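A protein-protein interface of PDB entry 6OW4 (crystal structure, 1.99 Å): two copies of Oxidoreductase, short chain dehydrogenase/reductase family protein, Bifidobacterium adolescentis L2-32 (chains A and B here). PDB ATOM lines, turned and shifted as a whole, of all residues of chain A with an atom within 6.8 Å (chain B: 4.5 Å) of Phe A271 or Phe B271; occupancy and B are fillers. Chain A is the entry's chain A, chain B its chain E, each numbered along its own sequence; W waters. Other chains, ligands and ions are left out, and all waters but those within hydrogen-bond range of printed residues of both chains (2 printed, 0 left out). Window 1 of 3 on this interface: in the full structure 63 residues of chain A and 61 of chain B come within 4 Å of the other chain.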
ATOM      1  N   LYS A  36     -26.611 -23.286 -12.121  1.00  0.00           N
ATOM      2  CA  LYS A  36     -27.178 -22.452 -11.025  1.00  0.00           C
ATOM      3  C   LYS A  36     -26.053 -21.771 -10.232  1.00  0.00           C
ATOM      4  O   LYS A  36     -26.345 -20.759  -9.561  1.00  0.00           O
ATOM      5  CB  LYS A  36     -28.054 -23.310 -10.106  1.00  0.00           C
ATOM      6  CG  LYS A  36     -29.330 -23.835 -10.749  1.00  0.00           C
ATOM      7  CD  LYS A  36     -30.040 -24.864  -9.907  1.00  0.00           C
ATOM      8  CE  LYS A  36     -31.507 -25.012 -10.255  1.00  0.00           C
ATOM      9  NZ  LYS A  36     -32.332 -23.960  -9.612  1.00  0.00           N
ATOM     10  N   PHE A  37     -24.827 -22.298 -10.305  1.00  0.00           N
ATOM     11  CA  PHE A  37     -23.631 -21.775  -9.589  1.00  0.00           C
ATOM     12  C   PHE A  37     -22.890 -20.746 -10.454  1.00  0.00           C
ATOM     13  O   PHE A  37     -21.927 -20.130  -9.950  1.00  0.00           O
ATOM     14  CB  PHE A  37     -22.714 -22.929  -9.177  1.00  0.00           C
ATOM     15  CG  PHE A  37     -23.350 -23.897  -8.211  1.00  0.00           C
ATOM     16  CD1 PHE A  37     -23.381 -23.627  -6.852  1.00  0.00           C
ATOM     17  CD2 PHE A  37     -23.937 -25.068  -8.667  1.00  0.00           C
ATOM     18  CE1 PHE A  37     -23.977 -24.515  -5.968  1.00  0.00           C
ATOM     19  CE2 PHE A  37     -24.530 -25.955  -7.783  1.00  0.00           C
ATOM     20  CZ  PHE A  37     -24.548 -25.677  -6.435  1.00  0.00           C
ATOM     21  N   LEU A  61     -16.368 -15.346  -7.082  1.00  0.00           N
ATOM     22  CA  LEU A  61     -17.493 -14.726  -7.836  1.00  0.00           C
ATOM     23  C   LEU A  61     -17.028 -14.352  -9.249  1.00  0.00           C
ATOM     24  O   LEU A  61     -17.801 -14.584 -10.199  1.00  0.00           O
ATOM     25  CB  LEU A  61     -17.995 -13.501  -7.066  1.00  0.00           C
ATOM     26  CG  LEU A  61     -18.697 -13.818  -5.748  1.00  0.00           C
ATOM     27  CD1 LEU A  61     -18.672 -12.625  -4.805  1.00  0.00           C
ATOM     28  CD2 LEU A  61     -20.125 -14.275  -5.997  1.00  0.00           C
ATOM     29  N   SER A 175     -28.820 -10.556  -4.376  1.00  0.00           N
ATOM     30  CA  SER A 175     -28.509 -11.350  -3.161  1.00  0.00           C
ATOM     31  C   SER A 175     -27.548 -10.571  -2.258  1.00  0.00           C
ATOM     32  O   SER A 175     -26.433 -10.261  -2.712  1.00  0.00           O
ATOM     33  CB  SER A 175     -27.943 -12.695  -3.532  1.00  0.00           C
ATOM     34  OG  SER A 175     -27.872 -13.541  -2.394  1.00  0.00           O
ATOM     35  N   ARG A 224     -32.784 -11.336  -1.994  1.00  0.00           N
ATOM     36  CA  ARG A 224     -32.518 -12.299  -0.894  1.00  0.00           C
ATOM     37  C   ARG A 224     -31.437 -11.715   0.020  1.00  0.00           C
ATOM     38  O   ARG A 224     -30.508 -11.060  -0.497  1.00  0.00           O
ATOM     39  CB  ARG A 224     -32.138 -13.664  -1.473  1.00  0.00           C
ATOM     40  CG  ARG A 224     -33.259 -14.312  -2.274  1.00  0.00           C
ATOM     41  CD  ARG A 224     -32.947 -15.719  -2.746  1.00  0.00           C
ATOM     42  NE  ARG A 224     -31.758 -15.775  -3.589  1.00  0.00           N
ATOM     43  CZ  ARG A 224     -30.540 -16.150  -3.199  1.00  0.00           C
ATOM     44  NH1 ARG A 224     -30.306 -16.531  -1.953  1.00  0.00           N
ATOM     45  NH2 ARG A 224     -29.549 -16.152  -4.076  1.00  0.00           N
ATOM     46  N   GLU A 264     -13.114 -22.017   1.664  1.00  0.00           N
ATOM     47  CA  GLU A 264     -14.269 -22.711   2.296  1.00  0.00           C
ATOM     48  C   GLU A 264     -15.372 -21.698   2.626  1.00  0.00           C
ATOM     49  O   GLU A 264     -16.554 -22.096   2.637  1.00  0.00           O
ATOM     50  CB  GLU A 264     -13.798 -23.485   3.527  1.00  0.00           C
ATOM     51  CG  GLU A 264     -12.831 -24.601   3.183  1.00  0.00           C
ATOM     52  CD  GLU A 264     -12.325 -25.406   4.367  1.00  0.00           C
ATOM     53  OE1 GLU A 264     -11.806 -24.795   5.319  1.00  0.00           O
ATOM     54  OE2 GLU A 264     -12.458 -26.642   4.338  1.00  0.00           O
ATOM     55  N   ALA A 266     -15.438 -18.827   0.661  1.00  0.00           N
ATOM     56  CA  ALA A 266     -15.637 -18.349  -0.729  1.00  0.00           C
ATOM     57  C   ALA A 266     -16.680 -19.218  -1.447  1.00  0.00           C
ATOM     58  O   ALA A 266     -17.538 -18.647  -2.146  1.00  0.00           O
ATOM     59  CB  ALA A 266     -14.318 -18.336  -1.464  1.00  0.00           C
ATOM     60  N   SER A 267     -16.614 -20.542  -1.280  1.00  0.00           N
ATOM     61  CA  SER A 267     -17.571 -21.511  -1.880  1.00  0.00           C
ATOM     62  C   SER A 267     -18.983 -21.260  -1.332  1.00  0.00           C
ATOM     63  O   SER A 267     -19.945 -21.405  -2.110  1.00  0.00           O
ATOM     64  CB  SER A 267     -17.134 -22.938  -1.657  1.00  0.00           C
ATOM     65  OG  SER A 267     -16.872 -23.180  -0.284  1.00  0.00           O
ATOM     66  N   THR A 268     -19.097 -20.891  -0.051  1.00  0.00           N
ATOM     67  CA  THR A 268     -20.387 -20.616   0.639  1.00  0.00           C
ATOM     68  C   THR A 268     -20.982 -19.298   0.128  1.00  0.00           C
ATOM     69  O   THR A 268     -22.217 -19.235  -0.013  1.00  0.00           O
ATOM     70  CB  THR A 268     -20.233 -20.589   2.166  1.00  0.00           C
ATOM     71  OG1 THR A 268     -19.510 -21.748   2.588  1.00  0.00           O
ATOM     72  CG2 THR A 268     -21.564 -20.546   2.885  1.00  0.00           C
ATOM     73  N   VAL A 269     -20.142 -18.285  -0.120  1.00  0.00           N
ATOM     74  CA  VAL A 269     -20.567 -16.946  -0.636  1.00  0.00           C
ATOM     75  C   VAL A 269     -21.104 -17.120  -2.061  1.00  0.00           C
ATOM     76  O   VAL A 269     -22.097 -16.456  -2.397  1.00  0.00           O
ATOM     77  CB  VAL A 269     -19.421 -15.917  -0.586  1.00  0.00           C
ATOM     78  CG1 VAL A 269     -19.782 -14.625  -1.303  1.00  0.00           C
ATOM     79  CG2 VAL A 269     -18.989 -15.614   0.842  1.00  0.00           C
ATOM     80  N   LEU A 270     -20.464 -17.971  -2.865  1.00  0.00           N
ATOM     81  CA  LEU A 270     -20.894 -18.288  -4.253  1.00  0.00           C
ATOM     82  C   LEU A 270     -22.275 -18.953  -4.217  1.00  0.00           C
ATOM     83  O   LEU A 270     -23.126 -18.582  -5.040  1.00  0.00           O
ATOM     84  CB  LEU A 270     -19.856 -19.196  -4.920  1.00  0.00           C
ATOM     85  CG  LEU A 270     -20.173 -19.629  -6.354  1.00  0.00           C
ATOM     86  CD1 LEU A 270     -20.488 -18.431  -7.239  1.00  0.00           C
ATOM     87  CD2 LEU A 270     -19.025 -20.432  -6.944  1.00  0.00           C
ATOM     88  N   PHE A 271     -22.489 -19.896  -3.296  1.00  0.00           N
ATOM     89  CA  PHE A 271     -23.780 -20.611  -3.119  1.00  0.00           C
ATOM     90  C   PHE A 271     -24.902 -19.594  -2.861  1.00  0.00           C
ATOM     91  O   PHE A 271     -25.903 -19.617  -3.603  1.00  0.00           O
ATOM     92  CB  PHE A 271     -23.686 -21.648  -1.995  1.00  0.00           C
ATOM     93  CG  PHE A 271     -25.006 -22.282  -1.638  1.00  0.00           C
ATOM     94  CD1 PHE A 271     -25.684 -23.069  -2.555  1.00  0.00           C
ATOM     95  CD2 PHE A 271     -25.581 -22.076  -0.393  1.00  0.00           C
ATOM     96  CE1 PHE A 271     -26.904 -23.642  -2.231  1.00  0.00           C
ATOM     97  CE2 PHE A 271     -26.801 -22.650  -0.070  1.00  0.00           C
ATOM     98  CZ  PHE A 271     -27.459 -23.433  -0.990  1.00  0.00           C
ATOM     99  N   LEU A 272     -24.729 -18.724  -1.859  1.00  0.00           N
ATOM    100  CA  LEU A 272     -25.751 -17.737  -1.404  1.00  0.00           C
ATOM    101  C   LEU A 272     -25.953 -16.636  -2.456  1.00  0.00           C
ATOM    102  O   LEU A 272     -27.095 -16.148  -2.571  1.00  0.00           O
ATOM    103  CB  LEU A 272     -25.327 -17.132  -0.061  1.00  0.00           C
ATOM    104  CG  LEU A 272     -25.528 -18.028   1.162  1.00  0.00           C
ATOM    105  CD1 LEU A 272     -24.962 -17.370   2.412  1.00  0.00           C
ATOM    106  CD2 LEU A 272     -26.999 -18.361   1.362  1.00  0.00           C
ATOM    107  N   ALA A 273     -24.897 -16.246  -3.178  1.00  0.00           N
ATOM    108  CA  ALA A 273     -24.931 -15.193  -4.222  1.00  0.00           C
ATOM    109  C   ALA A 273     -25.609 -15.727  -5.490  1.00  0.00           C
ATOM    110  O   ALA A 273     -26.357 -14.962  -6.123  1.00  0.00           O
ATOM    111  CB  ALA A 273     -23.537 -14.697  -4.518  1.00  0.00           C
ATOM    112  N   SER A 274     -25.356 -16.992  -5.838  1.00  0.00           N
ATOM    113  CA  SER A 274     -25.848 -17.653  -7.076  1.00  0.00           C
ATOM    114  C   SER A 274     -27.296 -18.130  -6.897  1.00  0.00           C
ATOM    115  O   SER A 274     -27.834 -18.015  -5.774  1.00  0.00           O
ATOM    116  CB  SER A 274     -24.936 -18.786  -7.479  1.00  0.00           C
ATOM    117  OG  SER A 274     -25.011 -19.861  -6.553  1.00  0.00           O
ATOM    118  N   ASP A 275     -27.888 -18.654  -7.975  1.00  0.00           N
ATOM    119  CA  ASP A 275     -29.302 -19.112  -8.039  1.00  0.00           C
ATOM    120  C   ASP A 275     -29.448 -20.490  -7.382  1.00  0.00           C
ATOM    121  O   ASP A 275     -30.602 -20.943  -7.228  1.00  0.00           O
ATOM    122  CB  ASP A 275     -29.795 -19.155  -9.486  1.00  0.00           C
ATOM    123  CG  ASP A 275     -29.790 -17.802 -10.171  1.00  0.00           C
ATOM    124  OD1 ASP A 275     -30.033 -16.791  -9.476  1.00  0.00           O
ATOM    125  OD2 ASP A 275     -29.538 -17.769 -11.392  1.00  0.00           O
ATOM    126  N   ALA A 276     -28.335 -21.141  -7.027  1.00  0.00           N
ATOM    127  CA  ALA A 276     -28.316 -22.402  -6.248  1.00  0.00           C
ATOM    128  C   ALA A 276     -29.112 -22.213  -4.951  1.00  0.00           C
ATOM    129  O   ALA A 276     -29.751 -23.184  -4.500  1.00  0.00           O
ATOM    130  CB  ALA A 276     -26.892 -22.818  -5.969  1.00  0.00           C
ATOM    131  N   SER A 277     -29.083 -20.999  -4.390  1.00  0.00           N
ATOM    132  CA  SER A 277     -29.743 -20.618  -3.114  1.00  0.00           C
ATOM    133  C   SER A 277     -31.006 -19.792  -3.385  1.00  0.00           C
ATOM    134  O   SER A 277     -31.385 -19.002  -2.504  1.00  0.00           O
ATOM    135  CB  SER A 277     -28.774 -19.857  -2.248  1.00  0.00           C
ATOM    136  OG  SER A 277     -28.405 -18.639  -2.873  1.00  0.00           O
ATOM    137  N   SER A 278     -31.653 -19.994  -4.539  1.00  0.00           N
ATOM    138  CA  SER A 278     -32.783 -19.170  -5.047  1.00  0.00           C
ATOM    139  C   SER A 278     -33.955 -19.135  -4.054  1.00  0.00           C
ATOM    140  O   SER A 278     -34.684 -18.134  -4.067  1.00  0.00           O
ATOM    141  CB  SER A 278     -33.244 -19.647  -6.402  1.00  0.00           C
ATOM    142  OG  SER A 278     -33.429 -21.054  -6.409  1.00  0.00           O
ATOM    143  N   VAL A 280     -33.488 -19.631  -0.693  1.00  0.00           N
ATOM    144  CA  VAL A 280     -32.798 -19.451   0.618  1.00  0.00           C
ATOM    145  C   VAL A 280     -32.692 -17.950   0.911  1.00  0.00           C
ATOM    146  O   VAL A 280     -31.934 -17.253   0.201  1.00  0.00           O
ATOM    147  CB  VAL A 280     -31.413 -20.124   0.634  1.00  0.00           C
ATOM    148  CG1 VAL A 280     -30.773 -20.052   2.012  1.00  0.00           C
ATOM    149  CG2 VAL A 280     -31.476 -21.565   0.149  1.00  0.00           C
ATOM    150  N   ILE A 285     -25.910 -19.444   7.464  1.00  0.00           N
ATOM    151  CA  ILE A 285     -25.097 -20.671   7.215  1.00  0.00           C
ATOM    152  C   ILE A 285     -23.833 -20.591   8.078  1.00  0.00           C
ATOM    153  O   ILE A 285     -22.947 -19.774   7.757  1.00  0.00           O
ATOM    154  CB  ILE A 285     -24.788 -20.842   5.714  1.00  0.00           C
ATOM    155  CG1 ILE A 285     -26.079 -21.024   4.911  1.00  0.00           C
ATOM    156  CG2 ILE A 285     -23.818 -21.994   5.492  1.00  0.00           C
ATOM    157  CD1 ILE A 285     -25.876 -21.135   3.418  1.00  0.00           C
ATOM    158  N   VAL A 287     -20.297 -21.844   9.237  1.00  0.00           N
ATOM    159  CA  VAL A 287     -19.120 -22.479   8.580  1.00  0.00           C
ATOM    160  C   VAL A 287     -17.996 -22.499   9.623  1.00  0.00           C
ATOM    161  O   VAL A 287     -17.089 -21.647   9.539  1.00  0.00           O
ATOM    162  CB  VAL A 287     -18.739 -21.717   7.294  1.00  0.00           C
ATOM    163  CG1 VAL A 287     -17.697 -22.459   6.473  1.00  0.00           C
ATOM    164  CG2 VAL A 287     -19.962 -21.411   6.439  1.00  0.00           C
ATOM    165  N   PHE B  37     -17.784 -28.199  -6.537  1.00  0.00           N
ATOM    166  CA  PHE B  37     -19.203 -28.621  -6.692  1.00  0.00           C
ATOM    167  C   PHE B  37     -19.287 -29.940  -7.469  1.00  0.00           C
ATOM    168  O   PHE B  37     -20.382 -30.540  -7.507  1.00  0.00           O
ATOM    169  CB  PHE B  37     -20.012 -27.498  -7.346  1.00  0.00           C
ATOM    170  CG  PHE B  37     -20.053 -26.231  -6.531  1.00  0.00           C
ATOM    171  CD1 PHE B  37     -19.092 -25.249  -6.702  1.00  0.00           C
ATOM    172  CD2 PHE B  37     -21.032 -26.032  -5.569  1.00  0.00           C
ATOM    173  CE1 PHE B  37     -19.118 -24.089  -5.943  1.00  0.00           C
ATOM    174  CE2 PHE B  37     -21.057 -24.871  -4.811  1.00  0.00           C
ATOM    175  CZ  PHE B  37     -20.101 -23.901  -4.999  1.00  0.00           C
ATOM    176  N   SER B 267     -30.050 -28.352  -5.375  1.00  0.00           N
ATOM    177  CA  SER B 267     -28.836 -27.491  -5.415  1.00  0.00           C
ATOM    178  C   SER B 267     -28.254 -27.338  -4.002  1.00  0.00           C
ATOM    179  O   SER B 267     -27.012 -27.266  -3.883  1.00  0.00           O
ATOM    180  CB  SER B 267     -29.114 -26.149  -6.062  1.00  0.00           C
ATOM    181  OG  SER B 267     -30.238 -25.509  -5.474  1.00  0.00           O
ATOM    182  N   THR B 268     -29.110 -27.307  -2.974  1.00  0.00           N
ATOM    183  CA  THR B 268     -28.705 -27.246  -1.542  1.00  0.00           C
ATOM    184  C   THR B 268     -28.050 -28.573  -1.141  1.00  0.00           C
ATOM    185  O   THR B 268     -27.045 -28.534  -0.412  1.00  0.00           O
ATOM    186  CB  THR B 268     -29.891 -26.914  -0.628  1.00  0.00           C
ATOM    187  OG1 THR B 268     -30.575 -25.782  -1.170  1.00  0.00           O
ATOM    188  CG2 THR B 268     -29.468 -26.622   0.795  1.00  0.00           C
ATOM    189  N   VAL B 269     -28.602 -29.701  -1.597  1.00  0.00           N
ATOM    190  CA  VAL B 269     -28.051 -31.064  -1.327  1.00  0.00           C
ATOM    191  C   VAL B 269     -26.649 -31.152  -1.941  1.00  0.00           C
ATOM    192  O   VAL B 269     -25.724 -31.581  -1.224  1.00  0.00           O
ATOM    193  CB  VAL B 269     -28.979 -32.178  -1.852  1.00  0.00           C
ATOM    194  CG1 VAL B 269     -28.301 -33.543  -1.831  1.00  0.00           C
ATOM    195  CG2 VAL B 269     -30.286 -32.232  -1.077  1.00  0.00           C
ATOM    196  N   LEU B 270     -26.495 -30.754  -3.208  1.00  0.00           N
ATOM    197  CA  LEU B 270     -25.203 -30.817  -3.947  1.00  0.00           C
ATOM    198  C   LEU B 270     -24.144 -29.983  -3.214  1.00  0.00           C
ATOM    199  O   LEU B 270     -22.983 -30.433  -3.156  1.00  0.00           O
ATOM    200  CB  LEU B 270     -25.394 -30.320  -5.384  1.00  0.00           C
ATOM    201  CG  LEU B 270     -24.127 -30.275  -6.242  1.00  0.00           C
ATOM    202  CD1 LEU B 270     -23.434 -31.631  -6.281  1.00  0.00           C
ATOM    203  CD2 LEU B 270     -24.445 -29.805  -7.651  1.00  0.00           C
ATOM    204  N   PHE B 271     -24.525 -28.816  -2.685  1.00  0.00           N
ATOM    205  CA  PHE B 271     -23.641 -27.940  -1.872  1.00  0.00           C
ATOM    206  C   PHE B 271     -23.110 -28.725  -0.666  1.00  0.00           C
ATOM    207  O   PHE B 271     -21.883 -28.729  -0.450  1.00  0.00           O
ATOM    208  CB  PHE B 271     -24.371 -26.672  -1.423  1.00  0.00           C
ATOM    209  CG  PHE B 271     -23.561 -25.801  -0.496  1.00  0.00           C
ATOM    210  CD1 PHE B 271     -22.408 -25.174  -0.945  1.00  0.00           C
ATOM    211  CD2 PHE B 271     -23.934 -25.626   0.828  1.00  0.00           C
ATOM    212  CE1 PHE B 271     -21.652 -24.383  -0.093  1.00  0.00           C
ATOM    213  CE2 PHE B 271     -23.179 -24.831   1.677  1.00  0.00           C
ATOM    214  CZ  PHE B 271     -22.040 -24.210   1.214  1.00  0.00           C
ATOM    215  N   LEU B 272     -24.007 -29.381   0.078  1.00  0.00           N
ATOM    216  CA  LEU B 272     -23.686 -30.100   1.343  1.00  0.00           C
ATOM    217  C   LEU B 272     -22.955 -31.419   1.054  1.00  0.00           C
ATOM    218  O   LEU B 272     -22.156 -31.840   1.912  1.00  0.00           O
ATOM    219  CB  LEU B 272     -24.978 -30.344   2.129  1.00  0.00           C
ATOM    220  CG  LEU B 272     -25.618 -29.100   2.744  1.00  0.00           C
ATOM    221  CD1 LEU B 272     -26.872 -29.468   3.524  1.00  0.00           C
ATOM    222  CD2 LEU B 272     -24.633 -28.364   3.642  1.00  0.00           C
ATOM    223  N   ALA B 273     -23.216 -32.052  -0.094  1.00  0.00           N
ATOM    224  CA  ALA B 273     -22.615 -33.350  -0.487  1.00  0.00           C
ATOM    225  C   ALA B 273     -21.196 -33.131  -1.028  1.00  0.00           C
ATOM    226  O   ALA B 273     -20.379 -34.069  -0.926  1.00  0.00           O
ATOM    227  CB  ALA B 273     -23.492 -34.043  -1.502  1.00  0.00           C
ATOM    228  N   SER B 274     -20.914 -31.937  -1.566  1.00  0.00           N
ATOM    229  CA  SER B 274     -19.663 -31.595  -2.296  1.00  0.00           C
ATOM    230  C   SER B 274     -18.647 -30.920  -1.366  1.00  0.00           C
ATOM    231  O   SER B 274     -18.983 -30.660  -0.190  1.00  0.00           O
ATOM    232  CB  SER B 274     -19.966 -30.718  -3.484  1.00  0.00           C
ATOM    233  OG  SER B 274     -20.324 -29.405  -3.070  1.00  0.00           O
ATOM    234  N   ALA B 276     -17.647 -27.956  -1.676  1.00  0.00           N
ATOM    235  CA  ALA B 276     -18.136 -26.566  -1.513  1.00  0.00           C
ATOM    236  C   ALA B 276     -18.441 -26.286  -0.035  1.00  0.00           C
ATOM    237  O   ALA B 276     -18.344 -25.117   0.375  1.00  0.00           O
ATOM    238  CB  ALA B 276     -19.355 -26.341  -2.375  1.00  0.00           C
ATOM    239  N   SER B 277     -18.791 -27.321   0.735  1.00  0.00           N
ATOM    240  CA  SER B 277     -19.231 -27.228   2.152  1.00  0.00           C
ATOM    241  C   SER B 277     -18.249 -27.954   3.082  1.00  0.00           C
ATOM    242  O   SER B 277     -18.688 -28.391   4.163  1.00  0.00           O
ATOM    243  CB  SER B 277     -20.619 -27.792   2.287  1.00  0.00           C
ATOM    244  OG  SER B 277     -20.651 -29.136   1.834  1.00  0.00           O
ATOM    245  N   ILE B 285     -29.574 -25.917   7.074  1.00  0.00           N
ATOM    246  CA  ILE B 285     -29.817 -24.905   6.002  1.00  0.00           C
ATOM    247  C   ILE B 285     -31.320 -24.860   5.724  1.00  0.00           C
ATOM    248  O   ILE B 285     -31.852 -25.838   5.156  1.00  0.00           O
ATOM    249  CB  ILE B 285     -28.993 -25.212   4.735  1.00  0.00           C
ATOM    250  CG1 ILE B 285     -27.490 -25.168   5.030  1.00  0.00           C
ATOM    251  CG2 ILE B 285     -29.378 -24.272   3.601  1.00  0.00           C
ATOM    252  CD1 ILE B 285     -26.609 -25.347   3.814  1.00  0.00           C
HETATM  253  O   HOH W   1     -17.085 -24.933   3.330  1.00  0.00           O
HETATM  254  O   HOH W   2     -14.935 -25.258   0.149  1.00  0.00           O
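OG of Ser A267 sits at hydrogen-bond distance from O of Ala B276 (2.5 Å).
The backbone carbonyl oxygen (O) of Ala A276 sits at hydrogen-bond distance from the side-chain hydroxyl (OG) of Ser B267 (2.6 Å).
The backbone carbonyl oxygen of Phe A271 sits at hydrogen-bond distance from the side-chain hydroxyl of Ser A274, 3.1 Å away.
The side-chain hydroxyl of Ser B274 lies within hydrogen-bond range of the backbone carbonyl oxygen of Phe B271 (3.1 Å).
O of Lys A36 lies within hydrogen-bond range of N of Ala A276 (3.2 Å).
O of Glu A264 lies within hydrogen-bond range of OG1 of Thr A268 (3.0 Å).
O of Glu A264 lies within hydrogen-bond range of OG of Ser A267, at 3.1 Å.
O of Leu B270 is in hydrogen-bond range of OG of Ser B274, 2.9 Å away.
Among the printed residues, merely in contact across the chains: Phe A37 with Phe B37, Phe A37 with Ser B267, Phe A37 with Leu B270, Ser A267 with Phe B37, Ser A267 with Phe B271, Thr A268 with Phe B271, Leu A270 with Phe B37, Phe A271 with Ser B267, Phe A271 with Thr B268 and Phe A271 with Phe B271.
Of the printed residues of chain A, Phe B271 touches Ser A267, Thr A268 and Phe A271.
Of the printed residues of chain A, Leu B270 touches Phe A37.
Printed residues of chain B within 4 Å of Leu A270: Phe B37.
Of the printed residues of chain A, Thr B268 touches Phe A271.
Printed residues of chain A within 4 Å of Ala B276: Ser A267 (2.5 Å).
Of the printed residues of chain B, Phe A37 touches Phe B37, Ser B267 and Leu B270.
Ser B277 touches none of the printed residues of chain A.
Leu A272 touches none of the printed residues of chain B.
The nearest printed residue of chain B that does not touch Phe A271 is Ile B285 (4.7 Å).
The nearest printed residue of chain A that does not touch Phe B271 is Ile A285 (4.8 Å).
The nearest printed residue of chain A that does not touch Ala B276 is Glu A264 (4.2 Å).
Hydrophobic or aromatic side chains of chain B within 4 Å of the printed part of chain A: Phe B37, Leu B270 and Phe B271.
Printed residues of chain A that touch a printed residue of chain B: Phe A37, Ser A267, Thr A268, Leu A270, Phe A271 and Ala A276.
Hydrophobic or aromatic side chains of chain A that line the printed part of chain B: Phe A37, Leu A270 and Phe A271.
Along chain A the printed residues that touch a printed residue of chain B span positions 37 to 276.
Among the printed residues, 12 pairs touch across the chains.
Among the printed residues, no Asp or Glu carboxylate lies within 4 Å of a Lys or Arg side-chain nitrogen of the other chain.
Phe B37 touches its own counterpart, Phe A37.
Ser A267 touches Phe B271, and with the chains exchanged Phe A271 touches Ser B267.
Ser A267 touches Ala B276, and with the chains exchanged Ala A276 touches Ser B267.
Phe A271 touches its own counterpart, Phe B271.
Positions printed for both chains: 37, 267, 268, 269, 270, 271, 272, 273, 274, 276, 277 and 285.
Of the 12 pairs that touch across the chains among the printed residues, 12 have their exchanged pair printed and touching as well.
Water W2 bridges the side-chain hydroxyl of Ser A267 and the backbone carbonyl oxygen of Ala B276.
Water W1 bridges the backbone carbonyl oxygen of Glu A264 and the backbone carbonyl oxygen of Ala B276.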
